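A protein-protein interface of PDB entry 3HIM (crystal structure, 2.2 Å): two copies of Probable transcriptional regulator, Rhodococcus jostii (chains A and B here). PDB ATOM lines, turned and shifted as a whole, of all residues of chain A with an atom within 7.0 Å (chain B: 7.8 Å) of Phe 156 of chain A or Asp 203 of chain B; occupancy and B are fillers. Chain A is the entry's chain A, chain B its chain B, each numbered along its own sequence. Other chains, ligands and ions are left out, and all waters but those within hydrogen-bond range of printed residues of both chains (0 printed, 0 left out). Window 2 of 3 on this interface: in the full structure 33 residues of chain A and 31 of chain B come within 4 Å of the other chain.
The backbone carbonyl oxygen (O) of His 154 of chain A sits at hydrogen-bond distance from the guanidinium group (NH2) of Arg 197 of chain B, at 2.8 Å. The guanidinium group (NH1) of Arg 197 of chain B lies within hydrogen-bond range of the backbone carbonyl oxygen (O) of Met 198 of chain A (3.3 Å). The backbone NH (N) of Gly 200 of chain A sits close to the guanidinium group (NH1) of Arg 197 of chain B, at 3.2 Å.
1 position is printed for both chains. Of the 11 pairs that touch across the chains among the printed residues, none has its exchanged pair printed and touching as well.
Of the 12 printed residues of chain B, 5 touch a printed residue of chain A. Hydrophobic or aromatic side chains of chain B within 4 Å of the printed part of chain A: Leu 194. Hydrophobic or aromatic side chains of chain A within 4 Å of the printed part of chain B: Phe 156, Ala 160 and Met 198. Among the printed residues, 11 pairs touch across the chains. Among the printed residues, no Asp or Glu carboxylate lies within 4 Å of a Lys or Arg side-chain nitrogen of the other chain.
Of chain B, only Glu 193, Arg 197 and Asp 203 come within 4 Å of Phe 156 of chain A. Glu 159 of chain A touches none of the printed residues of chain B. Printed residues of chain B within 4 Å of Met 198 of chain A: Leu 194 (3.8 Å) and Arg 197 (3.3 Å). Of the printed residues of chain B, Gly 200 of chain A touches Arg 197. Ala 189 of chain B touches none of the printed residues of chain A. Printed residues of chain A within 4 Å of Glu 193 of chain B: Phe 156 (3.8 Å). Of the printed residues of chain A, Leu 194 of chain B touches Ala 160 and Met 198. Asp 203 of chain B touches one residue of chain A.
O of Val 199 of chain A sits at hydrogen-bond distance from N of His 154 of chain A. N of Glu 159 of chain A sits at hydrogen-bond distance from OD1 of Asp 157 of chain A. The backbone NH (N) of Ala 160 of chain A is in hydrogen-bond range of the side-chain carboxylate (OD1) of Asp 157 of chain A, 2.8 Å away. The side-chain carboxylate (OE2) of Glu 193 of chain B is in salt-bridge range of the guanidinium group (NH2) of Arg 190 of chain B (2.8 Å). OD2 of Asp 203 of chain B lies within salt-bridge range of NH2 of Arg 197 of chain B (2.9 Å).
Among the printed residues, pairs that only touch across the chains: Phe 156 of chain A with Glu 193 of chain B, Phe 156 of chain A with Arg 197 of chain B, Phe 156 of chain A with Asp 203 of chain B, Asp 157 of chain A with Arg 190 of chain B, Ala 160 of chain A with Arg 190 of chain B, Ala 160 of chain A with Leu 194 of chain B, Met 198 of chain A with Leu 194 of chain B and Val 199 of chain A with Arg 197 of chain B.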
ATOM      1  N   HIS A 154      -7.308   1.834  -7.230  1.00  0.00           N
ATOM      2  CA  HIS A 154      -5.866   1.738  -7.223  1.00  0.00           C
ATOM      3  C   HIS A 154      -5.383   0.907  -6.049  1.00  0.00           C
ATOM      4  O   HIS A 154      -4.806   1.447  -5.108  1.00  0.00           O
ATOM      5  CB  HIS A 154      -5.262   3.137  -7.224  1.00  0.00           C
ATOM      6  CG  HIS A 154      -5.609   3.918  -8.452  1.00  0.00           C
ATOM      7  ND1 HIS A 154      -6.822   4.559  -8.611  1.00  0.00           N
ATOM      8  CD2 HIS A 154      -4.920   4.127  -9.599  1.00  0.00           C
ATOM      9  CE1 HIS A 154      -6.852   5.150  -9.791  1.00  0.00           C
ATOM     10  NE2 HIS A 154      -5.711   4.905 -10.409  1.00  0.00           N
ATOM     11  N   PRO A 155      -5.628  -0.422  -6.098  1.00  0.00           N
ATOM     12  CA  PRO A 155      -5.305  -1.288  -4.965  1.00  0.00           C
ATOM     13  C   PRO A 155      -3.796  -1.491  -4.770  1.00  0.00           C
ATOM     14  O   PRO A 155      -3.044  -1.495  -5.744  1.00  0.00           O
ATOM     15  CB  PRO A 155      -6.003  -2.612  -5.320  1.00  0.00           C
ATOM     16  CG  PRO A 155      -6.102  -2.603  -6.818  1.00  0.00           C
ATOM     17  CD  PRO A 155      -6.250  -1.169  -7.214  1.00  0.00           C
ATOM     18  N   PHE A 156      -3.365  -1.592  -3.513  1.00  0.00           N
ATOM     19  CA  PHE A 156      -1.999  -1.987  -3.168  1.00  0.00           C
ATOM     20  C   PHE A 156      -1.844  -3.478  -3.528  1.00  0.00           C
ATOM     21  O   PHE A 156      -0.884  -3.889  -4.167  1.00  0.00           O
ATOM     22  CB  PHE A 156      -1.746  -1.850  -1.652  1.00  0.00           C
ATOM     23  CG  PHE A 156      -1.262  -0.484  -1.193  1.00  0.00           C
ATOM     24  CD1 PHE A 156       0.052  -0.066  -1.430  1.00  0.00           C
ATOM     25  CD2 PHE A 156      -2.096   0.345  -0.427  1.00  0.00           C
ATOM     26  CE1 PHE A 156       0.515   1.204  -0.964  1.00  0.00           C
ATOM     27  CE2 PHE A 156      -1.653   1.600   0.041  1.00  0.00           C
ATOM     28  CZ  PHE A 156      -0.341   2.033  -0.232  1.00  0.00           C
ATOM     29  N   ASP A 157      -2.790  -4.294  -3.089  1.00  0.00           N
ATOM     30  CA  ASP A 157      -2.629  -5.739  -3.175  1.00  0.00           C
ATOM     31  C   ASP A 157      -4.012  -6.331  -3.269  1.00  0.00           C
ATOM     32  O   ASP A 157      -4.775  -6.314  -2.299  1.00  0.00           O
ATOM     33  CB  ASP A 157      -1.892  -6.265  -1.938  1.00  0.00           C
ATOM     34  CG  ASP A 157      -1.606  -7.759  -2.009  1.00  0.00           C
ATOM     35  OD1 ASP A 157      -2.534  -8.550  -2.281  1.00  0.00           O
ATOM     36  OD2 ASP A 157      -0.437  -8.152  -1.777  1.00  0.00           O
ATOM     37  N   ILE A 158      -4.330  -6.857  -4.445  1.00  0.00           N
ATOM     38  CA  ILE A 158      -5.695  -7.311  -4.730  1.00  0.00           C
ATOM     39  C   ILE A 158      -6.099  -8.492  -3.852  1.00  0.00           C
ATOM     40  O   ILE A 158      -7.172  -8.470  -3.241  1.00  0.00           O
ATOM     41  CB  ILE A 158      -5.911  -7.557  -6.247  1.00  0.00           C
ATOM     42  CG1 ILE A 158      -5.832  -6.199  -6.983  1.00  0.00           C
ATOM     43  CG2 ILE A 158      -7.220  -8.337  -6.508  1.00  0.00           C
ATOM     44  CD1 ILE A 158      -6.040  -6.264  -8.490  1.00  0.00           C
ATOM     45  N   GLU A 159      -5.233  -9.495  -3.745  1.00  0.00           N
ATOM     46  CA  GLU A 159      -5.540 -10.649  -2.883  1.00  0.00           C
ATOM     47  C   GLU A 159      -5.746 -10.213  -1.424  1.00  0.00           C
ATOM     48  O   GLU A 159      -6.646 -10.710  -0.739  1.00  0.00           O
ATOM     49  CB  GLU A 159      -4.466 -11.744  -2.991  1.00  0.00           C
ATOM     50  CG  GLU A 159      -4.587 -12.830  -1.916  1.00  0.00           C
ATOM     51  CD  GLU A 159      -3.763 -14.103  -2.187  1.00  0.00           C
ATOM     52  OE1 GLU A 159      -2.853 -14.103  -3.051  1.00  0.00           O
ATOM     53  OE2 GLU A 159      -4.026 -15.127  -1.503  1.00  0.00           O
ATOM     54  N   ALA A 160      -4.922  -9.270  -0.958  1.00  0.00           N
ATOM     55  CA  ALA A 160      -4.993  -8.836   0.426  1.00  0.00           C
ATOM     56  C   ALA A 160      -6.330  -8.143   0.726  1.00  0.00           C
ATOM     57  O   ALA A 160      -6.944  -8.389   1.782  1.00  0.00           O
ATOM     58  CB  ALA A 160      -3.837  -7.931   0.758  1.00  0.00           C
ATOM     59  N   ALA A 161      -6.759  -7.272  -0.196  1.00  0.00           N
ATOM     60  CA  ALA A 161      -8.037  -6.560  -0.075  1.00  0.00           C
ATOM     61  C   ALA A 161      -9.244  -7.509  -0.110  1.00  0.00           C
ATOM     62  O   ALA A 161     -10.155  -7.355   0.705  1.00  0.00           O
ATOM     63  CB  ALA A 161      -8.181  -5.482  -1.159  1.00  0.00           C
ATOM     64  N   MET A 198     -10.515   0.872   0.846  1.00  0.00           N
ATOM     65  CA  MET A 198      -9.461  -0.126   0.860  1.00  0.00           C
ATOM     66  C   MET A 198      -8.795  -0.222  -0.506  1.00  0.00           C
ATOM     67  O   MET A 198      -7.573  -0.247  -0.594  1.00  0.00           O
ATOM     68  CB  MET A 198     -10.015  -1.496   1.265  1.00  0.00           C
ATOM     69  CG  MET A 198     -10.028  -1.761   2.762  1.00  0.00           C
ATOM     70  SD  MET A 198     -10.468  -3.498   3.036  1.00  0.00           S
ATOM     71  CE  MET A 198     -12.090  -3.253   3.734  1.00  0.00           C
ATOM     72  N   VAL A 199      -9.602  -0.246  -1.562  1.00  0.00           N
ATOM     73  CA  VAL A 199      -9.104  -0.476  -2.920  1.00  0.00           C
ATOM     74  C   VAL A 199      -8.732   0.805  -3.683  1.00  0.00           C
ATOM     75  O   VAL A 199      -8.341   0.751  -4.850  1.00  0.00           O
ATOM     76  CB  VAL A 199     -10.108  -1.280  -3.755  1.00  0.00           C
ATOM     77  CG1 VAL A 199     -10.335  -2.630  -3.131  1.00  0.00           C
ATOM     78  CG2 VAL A 199     -11.413  -0.500  -3.926  1.00  0.00           C
ATOM     79  N   GLY A 200      -8.863   1.947  -3.022  1.00  0.00           N
ATOM     80  CA  GLY A 200      -8.380   3.211  -3.569  1.00  0.00           C
ATOM     81  C   GLY A 200      -9.415   3.916  -4.404  1.00  0.00           C
ATOM     82  O   GLY A 200      -9.091   4.554  -5.400  1.00  0.00           O
ATOM     83  N   PRO B  90      -0.470   8.397  11.718  1.00  0.00           N
ATOM     84  CA  PRO B  90      -0.347   7.263  10.785  1.00  0.00           C
ATOM     85  C   PRO B  90       0.654   6.204  11.238  1.00  0.00           C
ATOM     86  O   PRO B  90       0.392   5.010  11.051  1.00  0.00           O
ATOM     87  CB  PRO B  90       0.095   7.917   9.483  1.00  0.00           C
ATOM     88  CG  PRO B  90      -0.365   9.344   9.603  1.00  0.00           C
ATOM     89  CD  PRO B  90      -0.165   9.674  11.042  1.00  0.00           C
ATOM     90  N   ALA B 189       1.673  -6.479   7.475  1.00  0.00           N
ATOM     91  CA  ALA B 189       2.056  -5.431   6.538  1.00  0.00           C
ATOM     92  C   ALA B 189       0.908  -5.137   5.586  1.00  0.00           C
ATOM     93  O   ALA B 189       0.594  -3.974   5.322  1.00  0.00           O
ATOM     94  CB  ALA B 189       3.324  -5.817   5.759  1.00  0.00           C
ATOM     95  N   ARG B 190       0.283  -6.195   5.076  1.00  0.00           N
ATOM     96  CA  ARG B 190      -0.897  -6.049   4.217  1.00  0.00           C
ATOM     97  C   ARG B 190      -2.056  -5.324   4.907  1.00  0.00           C
ATOM     98  O   ARG B 190      -2.722  -4.462   4.305  1.00  0.00           O
ATOM     99  CB  ARG B 190      -1.352  -7.416   3.732  1.00  0.00           C
ATOM    100  CG  ARG B 190      -1.135  -7.655   2.269  1.00  0.00           C
ATOM    101  CD  ARG B 190       0.299  -7.826   1.884  1.00  0.00           C
ATOM    102  NE  ARG B 190       1.045  -6.560   1.810  1.00  0.00           N
ATOM    103  CZ  ARG B 190       2.369  -6.518   1.874  1.00  0.00           C
ATOM    104  NH1 ARG B 190       3.039  -7.660   1.981  1.00  0.00           N
ATOM    105  NH2 ARG B 190       3.022  -5.369   1.837  1.00  0.00           N
ATOM    106  N   VAL B 192      -1.812  -3.387   7.569  1.00  0.00           N
ATOM    107  CA  VAL B 192      -1.413  -1.993   7.795  1.00  0.00           C
ATOM    108  C   VAL B 192      -1.784  -1.099   6.595  1.00  0.00           C
ATOM    109  O   VAL B 192      -2.365  -0.030   6.776  1.00  0.00           O
ATOM    110  CB  VAL B 192       0.083  -1.869   8.108  1.00  0.00           C
ATOM    111  CG1 VAL B 192       0.533  -0.427   7.976  1.00  0.00           C
ATOM    112  CG2 VAL B 192       0.360  -2.391   9.515  1.00  0.00           C
ATOM    113  N   GLU B 193      -1.455  -1.544   5.379  1.00  0.00           N
ATOM    114  CA  GLU B 193      -1.788  -0.780   4.163  1.00  0.00           C
ATOM    115  C   GLU B 193      -3.289  -0.513   4.062  1.00  0.00           C
ATOM    116  O   GLU B 193      -3.724   0.593   3.682  1.00  0.00           O
ATOM    117  CB  GLU B 193      -1.321  -1.525   2.917  1.00  0.00           C
ATOM    118  CG  GLU B 193       0.193  -1.544   2.788  1.00  0.00           C
ATOM    119  CD  GLU B 193       0.685  -2.703   1.944  1.00  0.00           C
ATOM    120  OE1 GLU B 193      -0.161  -3.472   1.410  1.00  0.00           O
ATOM    121  OE2 GLU B 193       1.917  -2.848   1.834  1.00  0.00           O
ATOM    122  N   LEU B 194      -4.069  -1.539   4.397  1.00  0.00           N
ATOM    123  CA  LEU B 194      -5.529  -1.450   4.284  1.00  0.00           C
ATOM    124  C   LEU B 194      -6.146  -0.543   5.354  1.00  0.00           C
ATOM    125  O   LEU B 194      -7.057   0.221   5.050  1.00  0.00           O
ATOM    126  CB  LEU B 194      -6.162  -2.842   4.279  1.00  0.00           C
ATOM    127  CG  LEU B 194      -5.820  -3.693   3.049  1.00  0.00           C
ATOM    128  CD1 LEU B 194      -6.005  -5.197   3.362  1.00  0.00           C
ATOM    129  CD2 LEU B 194      -6.645  -3.283   1.821  1.00  0.00           C
ATOM    130  N   LEU B 196      -4.634   2.033   6.821  1.00  0.00           N
ATOM    131  CA  LEU B 196      -4.348   3.421   6.450  1.00  0.00           C
ATOM    132  C   LEU B 196      -5.324   3.873   5.387  1.00  0.00           C
ATOM    133  O   LEU B 196      -5.860   4.981   5.485  1.00  0.00           O
ATOM    134  CB  LEU B 196      -2.897   3.605   6.008  1.00  0.00           C
ATOM    135  CG  LEU B 196      -1.906   3.451   7.162  1.00  0.00           C
ATOM    136  CD1 LEU B 196      -0.481   3.334   6.608  1.00  0.00           C
ATOM    137  CD2 LEU B 196      -1.994   4.587   8.190  1.00  0.00           C
ATOM    138  N   ARG B 197      -5.598   3.007   4.409  1.00  0.00           N
ATOM    139  CA  ARG B 197      -6.542   3.329   3.344  1.00  0.00           C
ATOM    140  C   ARG B 197      -7.965   3.533   3.867  1.00  0.00           C
ATOM    141  O   ARG B 197      -8.674   4.448   3.426  1.00  0.00           O
ATOM    142  CB  ARG B 197      -6.529   2.253   2.252  1.00  0.00           C
ATOM    143  CG  ARG B 197      -5.370   2.365   1.288  1.00  0.00           C
ATOM    144  CD  ARG B 197      -5.740   3.276   0.140  1.00  0.00           C
ATOM    145  NE  ARG B 197      -4.727   3.357  -0.920  1.00  0.00           N
ATOM    146  CZ  ARG B 197      -4.765   2.684  -2.071  1.00  0.00           C
ATOM    147  NH1 ARG B 197      -5.741   1.829  -2.333  1.00  0.00           N
ATOM    148  NH2 ARG B 197      -3.809   2.864  -2.969  1.00  0.00           N
ATOM    149  N   GLY B 200      -8.524   6.784   5.388  1.00  0.00           N
ATOM    150  CA  GLY B 200      -8.335   7.815   4.368  1.00  0.00           C
ATOM    151  C   GLY B 200      -7.044   8.579   4.513  1.00  0.00           C
ATOM    152  O   GLY B 200      -6.983   9.761   4.178  1.00  0.00           O
ATOM    153  N   CYS B 201      -6.015   7.917   5.042  1.00  0.00           N
ATOM    154  CA  CYS B 201      -4.641   8.457   5.055  1.00  0.00           C
ATOM    155  C   CYS B 201      -4.007   8.380   3.654  1.00  0.00           C
ATOM    156  O   CYS B 201      -4.298   7.445   2.888  1.00  0.00           O
ATOM    157  CB  CYS B 201      -3.775   7.673   6.046  1.00  0.00           C
ATOM    158  SG  CYS B 201      -2.108   8.378   6.343  1.00  0.00           S
ATOM    159  N   ALA B 202      -3.142   9.349   3.327  1.00  0.00           N
ATOM    160  CA  ALA B 202      -2.344   9.296   2.089  1.00  0.00           C
ATOM    161  C   ALA B 202      -1.411   8.067   2.073  1.00  0.00           C
ATOM    162  O   ALA B 202      -1.029   7.554   3.132  1.00  0.00           O
ATOM    163  CB  ALA B 202      -1.550  10.604   1.885  1.00  0.00           C
ATOM    164  N   ASP B 203      -1.056   7.595   0.878  1.00  0.00           N
ATOM    165  CA  ASP B 203      -0.237   6.378   0.723  1.00  0.00           C
ATOM    166  C   ASP B 203       1.244   6.630   0.995  1.00  0.00           C
ATOM    167  O   ASP B 203       1.596   7.406   1.883  1.00  0.00           O
ATOM    168  CB  ASP B 203      -0.420   5.761  -0.677  1.00  0.00           C
ATOM    169  CG  ASP B 203      -1.874   5.379  -0.977  1.00  0.00           C
ATOM    170  OD1 ASP B 203      -2.703   5.334  -0.039  1.00  0.00           O
ATOM    171  OD2 ASP B 203      -2.186   5.123  -2.160  1.00  0.00           O
